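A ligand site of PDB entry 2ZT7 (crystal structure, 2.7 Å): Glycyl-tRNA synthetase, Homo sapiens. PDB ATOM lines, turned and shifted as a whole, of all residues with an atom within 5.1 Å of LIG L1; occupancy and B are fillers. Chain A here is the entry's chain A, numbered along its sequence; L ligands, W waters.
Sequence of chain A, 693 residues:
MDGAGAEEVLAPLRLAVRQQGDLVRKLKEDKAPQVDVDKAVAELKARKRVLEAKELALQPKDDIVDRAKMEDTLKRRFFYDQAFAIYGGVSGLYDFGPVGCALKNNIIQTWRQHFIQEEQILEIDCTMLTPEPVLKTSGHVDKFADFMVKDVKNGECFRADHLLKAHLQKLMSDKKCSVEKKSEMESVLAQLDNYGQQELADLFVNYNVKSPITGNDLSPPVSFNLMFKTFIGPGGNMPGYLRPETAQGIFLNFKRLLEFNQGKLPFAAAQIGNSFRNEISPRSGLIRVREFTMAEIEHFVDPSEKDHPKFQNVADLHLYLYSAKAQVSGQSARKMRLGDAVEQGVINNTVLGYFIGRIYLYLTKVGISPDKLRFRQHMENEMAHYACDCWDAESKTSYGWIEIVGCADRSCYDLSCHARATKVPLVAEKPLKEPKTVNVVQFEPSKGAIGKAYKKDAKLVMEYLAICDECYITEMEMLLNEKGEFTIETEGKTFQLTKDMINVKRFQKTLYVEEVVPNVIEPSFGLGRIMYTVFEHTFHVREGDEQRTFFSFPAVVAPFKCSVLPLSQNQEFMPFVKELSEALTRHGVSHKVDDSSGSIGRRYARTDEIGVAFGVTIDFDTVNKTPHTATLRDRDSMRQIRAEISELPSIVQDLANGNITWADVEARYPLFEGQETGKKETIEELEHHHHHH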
ATOM      1  N   ASP A 146      21.817   2.708  30.860  1.00  0.00           N
ATOM      2  CA  ASP A 146      22.178   3.503  32.026  1.00  0.00           C
ATOM      3  C   ASP A 146      21.886   2.694  33.271  1.00  0.00           C
ATOM      4  O   ASP A 146      20.950   1.901  33.303  1.00  0.00           O
ATOM      5  CB  ASP A 146      21.366   4.802  32.072  1.00  0.00           C
ATOM      6  CG  ASP A 146      21.980   5.915  31.250  1.00  0.00           C
ATOM      7  OD1 ASP A 146      21.357   6.988  31.141  1.00  0.00           O
ATOM      8  OD2 ASP A 146      23.093   5.714  30.711  1.00  0.00           O
ATOM      9  N   ARG A 159      18.188   7.216  37.877  1.00  0.00           N
ATOM     10  CA  ARG A 159      19.451   6.944  37.219  1.00  0.00           C
ATOM     11  C   ARG A 159      20.547   7.005  38.271  1.00  0.00           C
ATOM     12  O   ARG A 159      20.947   8.091  38.703  1.00  0.00           O
ATOM     13  CB  ARG A 159      19.737   7.962  36.114  1.00  0.00           C
ATOM     14  CG  ARG A 159      21.130   7.798  35.522  1.00  0.00           C
ATOM     15  CD  ARG A 159      21.373   8.677  34.307  1.00  0.00           C
ATOM     16  NE  ARG A 159      22.780   8.638  33.906  1.00  0.00           N
ATOM     17  CZ  ARG A 159      23.257   9.180  32.794  1.00  0.00           C
ATOM     18  NH1 ARG A 159      22.446   9.802  31.953  1.00  0.00           N
ATOM     19  NH2 ARG A 159      24.554   9.096  32.520  1.00  0.00           N
ATOM     20  N   ARG A 277      15.478   8.244  22.981  1.00  0.00           N
ATOM     21  CA  ARG A 277      16.220   7.737  24.133  1.00  0.00           C
ATOM     22  C   ARG A 277      15.215   7.582  25.274  1.00  0.00           C
ATOM     23  O   ARG A 277      14.751   8.568  25.837  1.00  0.00           O
ATOM     24  CB  ARG A 277      17.308   8.738  24.536  1.00  0.00           C
ATOM     25  CG  ARG A 277      18.181   9.200  23.375  1.00  0.00           C
ATOM     26  CD  ARG A 277      19.369   8.288  23.141  1.00  0.00           C
ATOM     27  NE  ARG A 277      20.558   8.749  23.843  1.00  0.00           N
ATOM     28  CZ  ARG A 277      21.654   9.199  23.251  1.00  0.00           C
ATOM     29  NH1 ARG A 277      21.716   9.242  21.925  1.00  0.00           N
ATOM     30  NH2 ARG A 277      22.690   9.604  23.962  1.00  0.00           N
ATOM     31  N   GLU A 279      15.010   7.645  28.146  1.00  0.00           N
ATOM     32  CA  GLU A 279      15.646   8.128  29.357  1.00  0.00           C
ATOM     33  C   GLU A 279      14.893   7.652  30.596  1.00  0.00           C
ATOM     34  O   GLU A 279      13.659   7.656  30.631  1.00  0.00           O
ATOM     35  CB  GLU A 279      15.697   9.667  29.342  1.00  0.00           C
ATOM     36  CG  GLU A 279      17.066  10.261  29.660  1.00  0.00           C
ATOM     37  CD  GLU A 279      18.125   9.897  28.628  1.00  0.00           C
ATOM     38  OE1 GLU A 279      17.888  10.128  27.421  1.00  0.00           O
ATOM     39  OE2 GLU A 279      19.205   9.390  29.021  1.00  0.00           O
ATOM     40  N   LEU A 286      14.606  20.670  28.895  1.00  0.00           N
ATOM     41  CA  LEU A 286      15.027  20.314  27.536  1.00  0.00           C
ATOM     42  C   LEU A 286      16.378  19.620  27.484  1.00  0.00           C
ATOM     43  O   LEU A 286      16.778  19.129  26.427  1.00  0.00           O
ATOM     44  CB  LEU A 286      15.067  21.565  26.649  1.00  0.00           C
ATOM     45  CG  LEU A 286      13.719  22.159  26.223  1.00  0.00           C
ATOM     46  CD1 LEU A 286      13.955  23.379  25.344  1.00  0.00           C
ATOM     47  CD2 LEU A 286      12.902  21.119  25.477  1.00  0.00           C
ATOM     48  N   ILE A 287      17.092  19.589  28.607  1.00  0.00           N
ATOM     49  CA  ILE A 287      18.396  18.931  28.648  1.00  0.00           C
ATOM     50  C   ILE A 287      18.251  17.423  28.527  1.00  0.00           C
ATOM     51  O   ILE A 287      19.091  16.749  27.931  1.00  0.00           O
ATOM     52  CB  ILE A 287      19.172  19.268  29.949  1.00  0.00           C
ATOM     53  CG1 ILE A 287      19.492  20.752  30.000  1.00  0.00           C
ATOM     54  CG2 ILE A 287      20.455  18.454  30.022  1.00  0.00           C
ATOM     55  CD1 ILE A 287      20.288  21.242  28.806  1.00  0.00           C
ATOM     56  N   ARG A 288      17.182  16.894  29.104  1.00  0.00           N
ATOM     57  CA  ARG A 288      16.913  15.461  29.064  1.00  0.00           C
ATOM     58  C   ARG A 288      15.540  15.153  28.498  1.00  0.00           C
ATOM     59  O   ARG A 288      14.536  15.240  29.201  1.00  0.00           O
ATOM     60  CB  ARG A 288      17.013  14.840  30.457  1.00  0.00           C
ATOM     61  CG  ARG A 288      18.411  14.446  30.840  1.00  0.00           C
ATOM     62  CD  ARG A 288      18.456  12.994  31.263  1.00  0.00           C
ATOM     63  NE  ARG A 288      19.593  12.307  30.676  1.00  0.00           N
ATOM     64  CZ  ARG A 288      20.855  12.688  30.829  1.00  0.00           C
ATOM     65  NH1 ARG A 288      21.142  13.756  31.571  1.00  0.00           N
ATOM     66  NH2 ARG A 288      21.827  12.018  30.247  1.00  0.00           N
ATOM     67  N   VAL A 289      15.499  14.788  27.226  1.00  0.00           N
ATOM     68  CA  VAL A 289      14.243  14.446  26.566  1.00  0.00           C
ATOM     69  C   VAL A 289      14.352  13.016  26.048  1.00  0.00           C
ATOM     70  O   VAL A 289      15.447  12.467  25.942  1.00  0.00           O
ATOM     71  CB  VAL A 289      13.957  15.402  25.387  1.00  0.00           C
ATOM     72  CG1 VAL A 289      13.736  16.810  25.912  1.00  0.00           C
ATOM     73  CG2 VAL A 289      15.103  15.376  24.399  1.00  0.00           C
ATOM     74  N   ARG A 290      13.205  12.427  25.733  1.00  0.00           N
ATOM     75  CA  ARG A 290      13.174  11.058  25.224  1.00  0.00           C
ATOM     76  C   ARG A 290      12.971  11.089  23.725  1.00  0.00           C
ATOM     77  O   ARG A 290      12.757  10.061  23.085  1.00  0.00           O
ATOM     78  CB  ARG A 290      12.034  10.300  25.905  1.00  0.00           C
ATOM     79  CG  ARG A 290      12.278  10.085  27.380  1.00  0.00           C
ATOM     80  CD  ARG A 290      11.052   9.626  28.129  1.00  0.00           C
ATOM     81  NE  ARG A 290      11.395   9.219  29.481  1.00  0.00           N
ATOM     82  CZ  ARG A 290      10.522   9.032  30.458  1.00  0.00           C
ATOM     83  NH1 ARG A 290       9.224   9.209  30.230  1.00  0.00           N
ATOM     84  NH2 ARG A 290      10.939   8.656  31.661  1.00  0.00           N
ATOM     85  N   PHE A 292      14.423  13.842  20.417  1.00  0.00           N
ATOM     86  CA  PHE A 292      15.080  15.084  20.025  1.00  0.00           C
ATOM     87  C   PHE A 292      15.689  15.030  18.639  1.00  0.00           C
ATOM     88  O   PHE A 292      15.917  13.961  18.078  1.00  0.00           O
ATOM     89  CB  PHE A 292      16.150  15.462  21.046  1.00  0.00           C
ATOM     90  CG  PHE A 292      17.186  14.394  21.253  1.00  0.00           C
ATOM     91  CD1 PHE A 292      16.891  13.253  21.993  1.00  0.00           C
ATOM     92  CD2 PHE A 292      18.460  14.518  20.714  1.00  0.00           C
ATOM     93  CE1 PHE A 292      17.838  12.261  22.200  1.00  0.00           C
ATOM     94  CE2 PHE A 292      19.427  13.527  20.911  1.00  0.00           C
ATOM     95  CZ  PHE A 292      19.110  12.390  21.649  1.00  0.00           C
ATOM     96  N   MET A 294      18.817  15.640  16.247  1.00  0.00           N
ATOM     97  CA  MET A 294      20.270  15.719  16.340  1.00  0.00           C
ATOM     98  C   MET A 294      20.908  15.696  14.961  1.00  0.00           C
ATOM     99  O   MET A 294      20.440  15.019  14.052  1.00  0.00           O
ATOM    100  CB  MET A 294      20.815  14.553  17.187  1.00  0.00           C
ATOM    101  CG  MET A 294      20.739  13.182  16.533  1.00  0.00           C
ATOM    102  SD  MET A 294      21.216  11.882  17.682  1.00  0.00           S
ATOM    103  CE  MET A 294      22.796  12.475  18.243  1.00  0.00           C
ATOM    104  N   TYR A 386      31.342   2.009  21.104  1.00  0.00           N
ATOM    105  CA  TYR A 386      31.821   2.109  19.728  1.00  0.00           C
ATOM    106  C   TYR A 386      33.002   3.059  19.559  1.00  0.00           C
ATOM    107  O   TYR A 386      33.493   3.233  18.447  1.00  0.00           O
ATOM    108  CB  TYR A 386      30.686   2.560  18.819  1.00  0.00           C
ATOM    109  CG  TYR A 386      29.944   3.785  19.335  1.00  0.00           C
ATOM    110  CD1 TYR A 386      30.603   5.006  19.485  1.00  0.00           C
ATOM    111  CD2 TYR A 386      28.605   3.700  19.707  1.00  0.00           C
ATOM    112  CE1 TYR A 386      29.931   6.114  20.005  1.00  0.00           C
ATOM    113  CE2 TYR A 386      27.929   4.804  20.218  1.00  0.00           C
ATOM    114  CZ  TYR A 386      28.603   6.009  20.369  1.00  0.00           C
ATOM    115  OH  TYR A 386      27.935   7.096  20.896  1.00  0.00           O
ATOM    116  N   ASP A 392      33.863  15.857  24.365  1.00  0.00           N
ATOM    117  CA  ASP A 392      32.535  16.440  24.407  1.00  0.00           C
ATOM    118  C   ASP A 392      32.609  17.938  24.654  1.00  0.00           C
ATOM    119  O   ASP A 392      33.405  18.404  25.462  1.00  0.00           O
ATOM    120  CB  ASP A 392      31.714  15.797  25.538  1.00  0.00           C
ATOM    121  CG  ASP A 392      31.324  14.368  25.243  1.00  0.00           C
ATOM    122  OD1 ASP A 392      30.727  13.722  26.124  1.00  0.00           O
ATOM    123  OD2 ASP A 392      31.605  13.886  24.123  1.00  0.00           O
ATOM    124  N   GLU A 403      27.135  17.863  28.357  1.00  0.00           N
ATOM    125  CA  GLU A 403      27.602  17.702  26.984  1.00  0.00           C
ATOM    126  C   GLU A 403      26.506  18.104  26.015  1.00  0.00           C
ATOM    127  O   GLU A 403      25.361  17.662  26.119  1.00  0.00           O
ATOM    128  CB  GLU A 403      28.043  16.246  26.729  1.00  0.00           C
ATOM    129  CG  GLU A 403      27.075  15.413  25.909  1.00  0.00           C
ATOM    130  CD  GLU A 403      27.620  14.025  25.581  1.00  0.00           C
ATOM    131  OE1 GLU A 403      27.846  13.234  26.523  1.00  0.00           O
ATOM    132  OE2 GLU A 403      27.819  13.729  24.384  1.00  0.00           O
ATOM    133  N   ILE A 404      26.860  18.960  25.056  1.00  0.00           N
ATOM    134  CA  ILE A 404      25.910  19.420  24.058  1.00  0.00           C
ATOM    135  C   ILE A 404      26.334  18.971  22.666  1.00  0.00           C
ATOM    136  O   ILE A 404      25.534  18.966  21.738  1.00  0.00           O
ATOM    137  CB  ILE A 404      25.770  20.963  24.092  1.00  0.00           C
ATOM    138  CG1 ILE A 404      27.129  21.630  23.909  1.00  0.00           C
ATOM    139  CG2 ILE A 404      25.144  21.396  25.414  1.00  0.00           C
ATOM    140  CD1 ILE A 404      27.090  23.138  23.955  1.00  0.00           C
ATOM    141  N   VAL A 405      27.607  18.584  22.541  1.00  0.00           N
ATOM    142  CA  VAL A 405      28.144  18.103  21.274  1.00  0.00           C
ATOM    143  C   VAL A 405      29.225  17.068  21.577  1.00  0.00           C
ATOM    144  O   VAL A 405      30.206  17.352  22.261  1.00  0.00           O
ATOM    145  CB  VAL A 405      28.793  19.240  20.449  1.00  0.00           C
ATOM    146  CG1 VAL A 405      29.248  18.711  19.101  1.00  0.00           C
ATOM    147  CG2 VAL A 405      27.817  20.391  20.270  1.00  0.00           C
ATOM    148  N   GLY A 406      29.051  15.859  21.058  1.00  0.00           N
ATOM    149  CA  GLY A 406      30.008  14.805  21.288  1.00  0.00           C
ATOM    150  C   GLY A 406      30.820  14.458  20.061  1.00  0.00           C
ATOM    151  O   GLY A 406      30.292  13.907  19.091  1.00  0.00           O
ATOM    152  N   SER A 524      28.720  14.765  16.902  1.00  0.00           N
ATOM    153  CA  SER A 524      27.282  14.606  17.141  1.00  0.00           C
ATOM    154  C   SER A 524      26.676  15.800  17.855  1.00  0.00           C
ATOM    155  O   SER A 524      27.015  16.094  19.003  1.00  0.00           O
ATOM    156  CB  SER A 524      27.035  13.334  17.951  1.00  0.00           C
ATOM    157  OG  SER A 524      25.655  13.067  18.063  1.00  0.00           O
ATOM    158  N   PHE A 525      25.752  16.494  17.174  1.00  0.00           N
ATOM    159  CA  PHE A 525      25.119  17.678  17.737  1.00  0.00           C
ATOM    160  C   PHE A 525      23.701  17.469  18.243  1.00  0.00           C
ATOM    161  O   PHE A 525      22.829  16.982  17.521  1.00  0.00           O
ATOM    162  CB  PHE A 525      25.102  18.809  16.703  1.00  0.00           C
ATOM    163  CG  PHE A 525      26.453  19.215  16.228  1.00  0.00           C
ATOM    164  CD1 PHE A 525      27.200  18.367  15.418  1.00  0.00           C
ATOM    165  CD2 PHE A 525      26.990  20.447  16.572  1.00  0.00           C
ATOM    166  CE1 PHE A 525      28.469  18.730  14.970  1.00  0.00           C
ATOM    167  CE2 PHE A 525      28.261  20.830  16.137  1.00  0.00           C
ATOM    168  CZ  PHE A 525      28.991  19.965  15.332  1.00  0.00           C
ATOM    169  N   GLY A 526      23.471  17.851  19.503  1.00  0.00           N
ATOM    170  CA  GLY A 526      22.148  17.743  20.084  1.00  0.00           C
ATOM    171  C   GLY A 526      21.532  19.125  19.990  1.00  0.00           C
ATOM    172  O   GLY A 526      21.636  19.924  20.912  1.00  0.00           O
ATOM    173  N   ARG A 529      19.834  20.599  23.224  1.00  0.00           N
ATOM    174  CA  ARG A 529      20.656  21.134  24.316  1.00  0.00           C
ATOM    175  C   ARG A 529      21.399  22.398  23.905  1.00  0.00           C
ATOM    176  O   ARG A 529      21.650  23.273  24.729  1.00  0.00           O
ATOM    177  CB  ARG A 529      21.665  20.087  24.782  1.00  0.00           C
ATOM    178  CG  ARG A 529      21.025  18.812  25.326  1.00  0.00           C
ATOM    179  CD  ARG A 529      22.070  17.926  25.993  1.00  0.00           C
ATOM    180  NE  ARG A 529      21.471  16.698  26.517  1.00  0.00           N
ATOM    181  CZ  ARG A 529      22.146  15.755  27.161  1.00  0.00           C
ATOM    182  NH1 ARG A 529      23.444  15.877  27.364  1.00  0.00           N
ATOM    183  NH2 ARG A 529      21.519  14.670  27.587  1.00  0.00           N
HETATM  184  P1  LIG L   1      24.272  11.921  28.432  1.00  0.00           P
HETATM  185  O1  LIG L   1      23.534  13.305  28.814  1.00  0.00           O
HETATM  186  O2  LIG L   1      23.359  10.766  28.481  1.00  0.00           O
HETATM  187  O3  LIG L   1      25.487  11.783  29.476  1.00  0.00           O
HETATM  188  P2  LIG L   1      25.292  10.891  26.057  1.00  0.00           P
HETATM  189  O4  LIG L   1      26.894  10.721  26.135  1.00  0.00           O
HETATM  190  O5  LIG L   1      24.572   9.659  26.452  1.00  0.00           O
HETATM  191  O6  LIG L   1      24.943  12.148  26.984  1.00  0.00           O
HETATM  192  P3  LIG L   1      25.992  10.935  23.352  1.00  0.00           P
HETATM  193  O7  LIG L   1      25.831   9.335  23.172  1.00  0.00           O
HETATM  194  O8  LIG L   1      27.384  11.316  23.669  1.00  0.00           O
HETATM  195  O9  LIG L   1      24.976  11.335  24.540  1.00  0.00           O
HETATM  196  O10 LIG L   1      25.452  11.585  21.981  1.00  0.00           O
HETATM  197  C1  LIG L   1      25.628  12.981  21.735  1.00  0.00           C
HETATM  198  C2  LIG L   1      24.623  13.788  22.564  1.00  0.00           C
HETATM  199  O11 LIG L   1      23.295  13.660  22.039  1.00  0.00           O
HETATM  200  C3  LIG L   1      24.801  15.308  22.503  1.00  0.00           C
HETATM  201  O12 LIG L   1      25.994  15.683  23.206  1.00  0.00           O
HETATM  202  C4  LIG L   1      23.541  15.670  23.289  1.00  0.00           C
HETATM  203  O13 LIG L   1      23.169  17.019  22.986  1.00  0.00           O
HETATM  204  C5  LIG L   1      22.529  14.703  22.662  1.00  0.00           C
HETATM  205  N1  LIG L   1      21.647  14.114  23.691  1.00  0.00           N
HETATM  206  C6  LIG L   1      21.841  12.946  24.297  1.00  0.00           C
HETATM  207  N2  LIG L   1      20.819  12.683  25.094  1.00  0.00           N
HETATM  208  C7  LIG L   1      19.962  13.693  25.002  1.00  0.00           C
HETATM  209  C8  LIG L   1      18.730  13.974  25.591  1.00  0.00           C
HETATM  210  N3  LIG L   1      18.172  13.108  26.430  1.00  0.00           N
HETATM  211  N4  LIG L   1      18.109  15.111  25.270  1.00  0.00           N
HETATM  212  C9  LIG L   1      18.642  15.962  24.415  1.00  0.00           C
HETATM  213  N5  LIG L   1      19.814  15.735  23.845  1.00  0.00           N
HETATM  214  C10 LIG L   1      20.491  14.607  24.108  1.00  0.00           C
HETATM  215  N1  LG2 L   2      25.975   8.643  17.397  1.00  0.00           N
HETATM  216  C1  LG2 L   2      26.792   8.773  18.637  1.00  0.00           C
HETATM  217  C2  LG2 L   2      26.143   9.665  19.667  1.00  0.00           C
HETATM  218  O1  LG2 L   2      26.432  10.877  19.675  1.00  0.00           O
HETATM  219  O2  LG2 L   2      25.340   9.154  20.486  1.00  0.00           O
HETATM  220  O   HOH W   1      22.030   9.055  27.249  1.00  0.00           O
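The side-chain hydroxyl (OG) of Ser 524 lies within hydrogen-bond range of an oxygen (O1) of LG2 L2 (2.8 Å).
N of Val 289 sits close to N4 of LIG L1, 3.3 Å away.
An oxygen (O2) of LIG L1 is in salt-bridge range of the guanidinium group (NH1) of Arg 159 (3.7 Å).
O1 of LIG L1 lies within salt-bridge range of NH2 of Arg 529 (2.7 Å).
OE2 of Glu 403 lies within hydrogen-bond range of O12 of LIG L1.
The guanidinium group (NH1) of Arg 277 lies within salt-bridge range of an oxygen (O2) of LG2 L2, 3.9 Å away.
The backbone NH (N) of Val 405 sits at hydrogen-bond distance from an oxygen (O12) of LIG L1, 3.4 Å away.
An oxygen (O2) of LG2 L2 lies close to the side-chain hydroxyl (OH) of Tyr 386 (3.3 Å).
A nitrogen (N3) of LIG L1 sits at hydrogen-bond distance from the backbone carbonyl oxygen (O) of Val 289 (2.8 Å).
O13 of LIG L1 sits at hydrogen-bond distance from O of Ile 404 (3.3 Å).
NH2 of Arg 277 is in salt-bridge range of O5 of LIG L1 (3.1 Å).
NH2 of Arg 288 lies within salt-bridge range of O1 of LIG L1.
OE1 of Glu 279 is in hydrogen-bond range of N3 of LIG L1, at 3.2 Å.
An oxygen (O10) of LIG L1 lies close to an oxygen (O1) of LG2 L2, at 2.6 Å.
OE2 of Glu 279 is in salt-bridge range of NE of Arg 288 (3.4 Å).
N of Gly 526 is in hydrogen-bond range of O of Ile 404 (3.2 Å).
The backbone carbonyl oxygen (O) of Arg 290 lies within hydrogen-bond range of the backbone NH (N) of Arg 277, at 3.3 Å.
The backbone NH (N) of Ser 524 is in hydrogen-bond range of the backbone carbonyl oxygen (O) of Gly 406 (2.8 Å).
The guanidinium group of Arg 159 is in salt-bridge range of the side-chain carboxylate of Asp 146 (3.1 Å).
O of Ile 287 is in hydrogen-bond range of NE of Arg 529, 2.8 Å away.
The backbone carbonyl oxygen of Glu 403 lies within hydrogen-bond range of the guanidinium group of Arg 529 (2.9 Å).
The backbone carbonyl oxygen (O) of Glu 279 sits at hydrogen-bond distance from the guanidinium group (NE) of Arg 290 (3.0 Å).
N4 of LIG L1 lies close to O of Ile 287 (3.3 Å).
Merely in contact with LIG L1: Phe 292, Tyr 386, Gly 406, Ser 524 and Gly 526.
Of the 21 residues printed, 15 come within 4 Å of LIG L1.
Water W1 lies within hydrogen-bond range of an oxygen (O2) of LIG L1 (2.5 Å), the side-chain carboxylate of Glu 279 (3.4 Å) and the guanidinium group of Arg 277 (3.4 Å).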
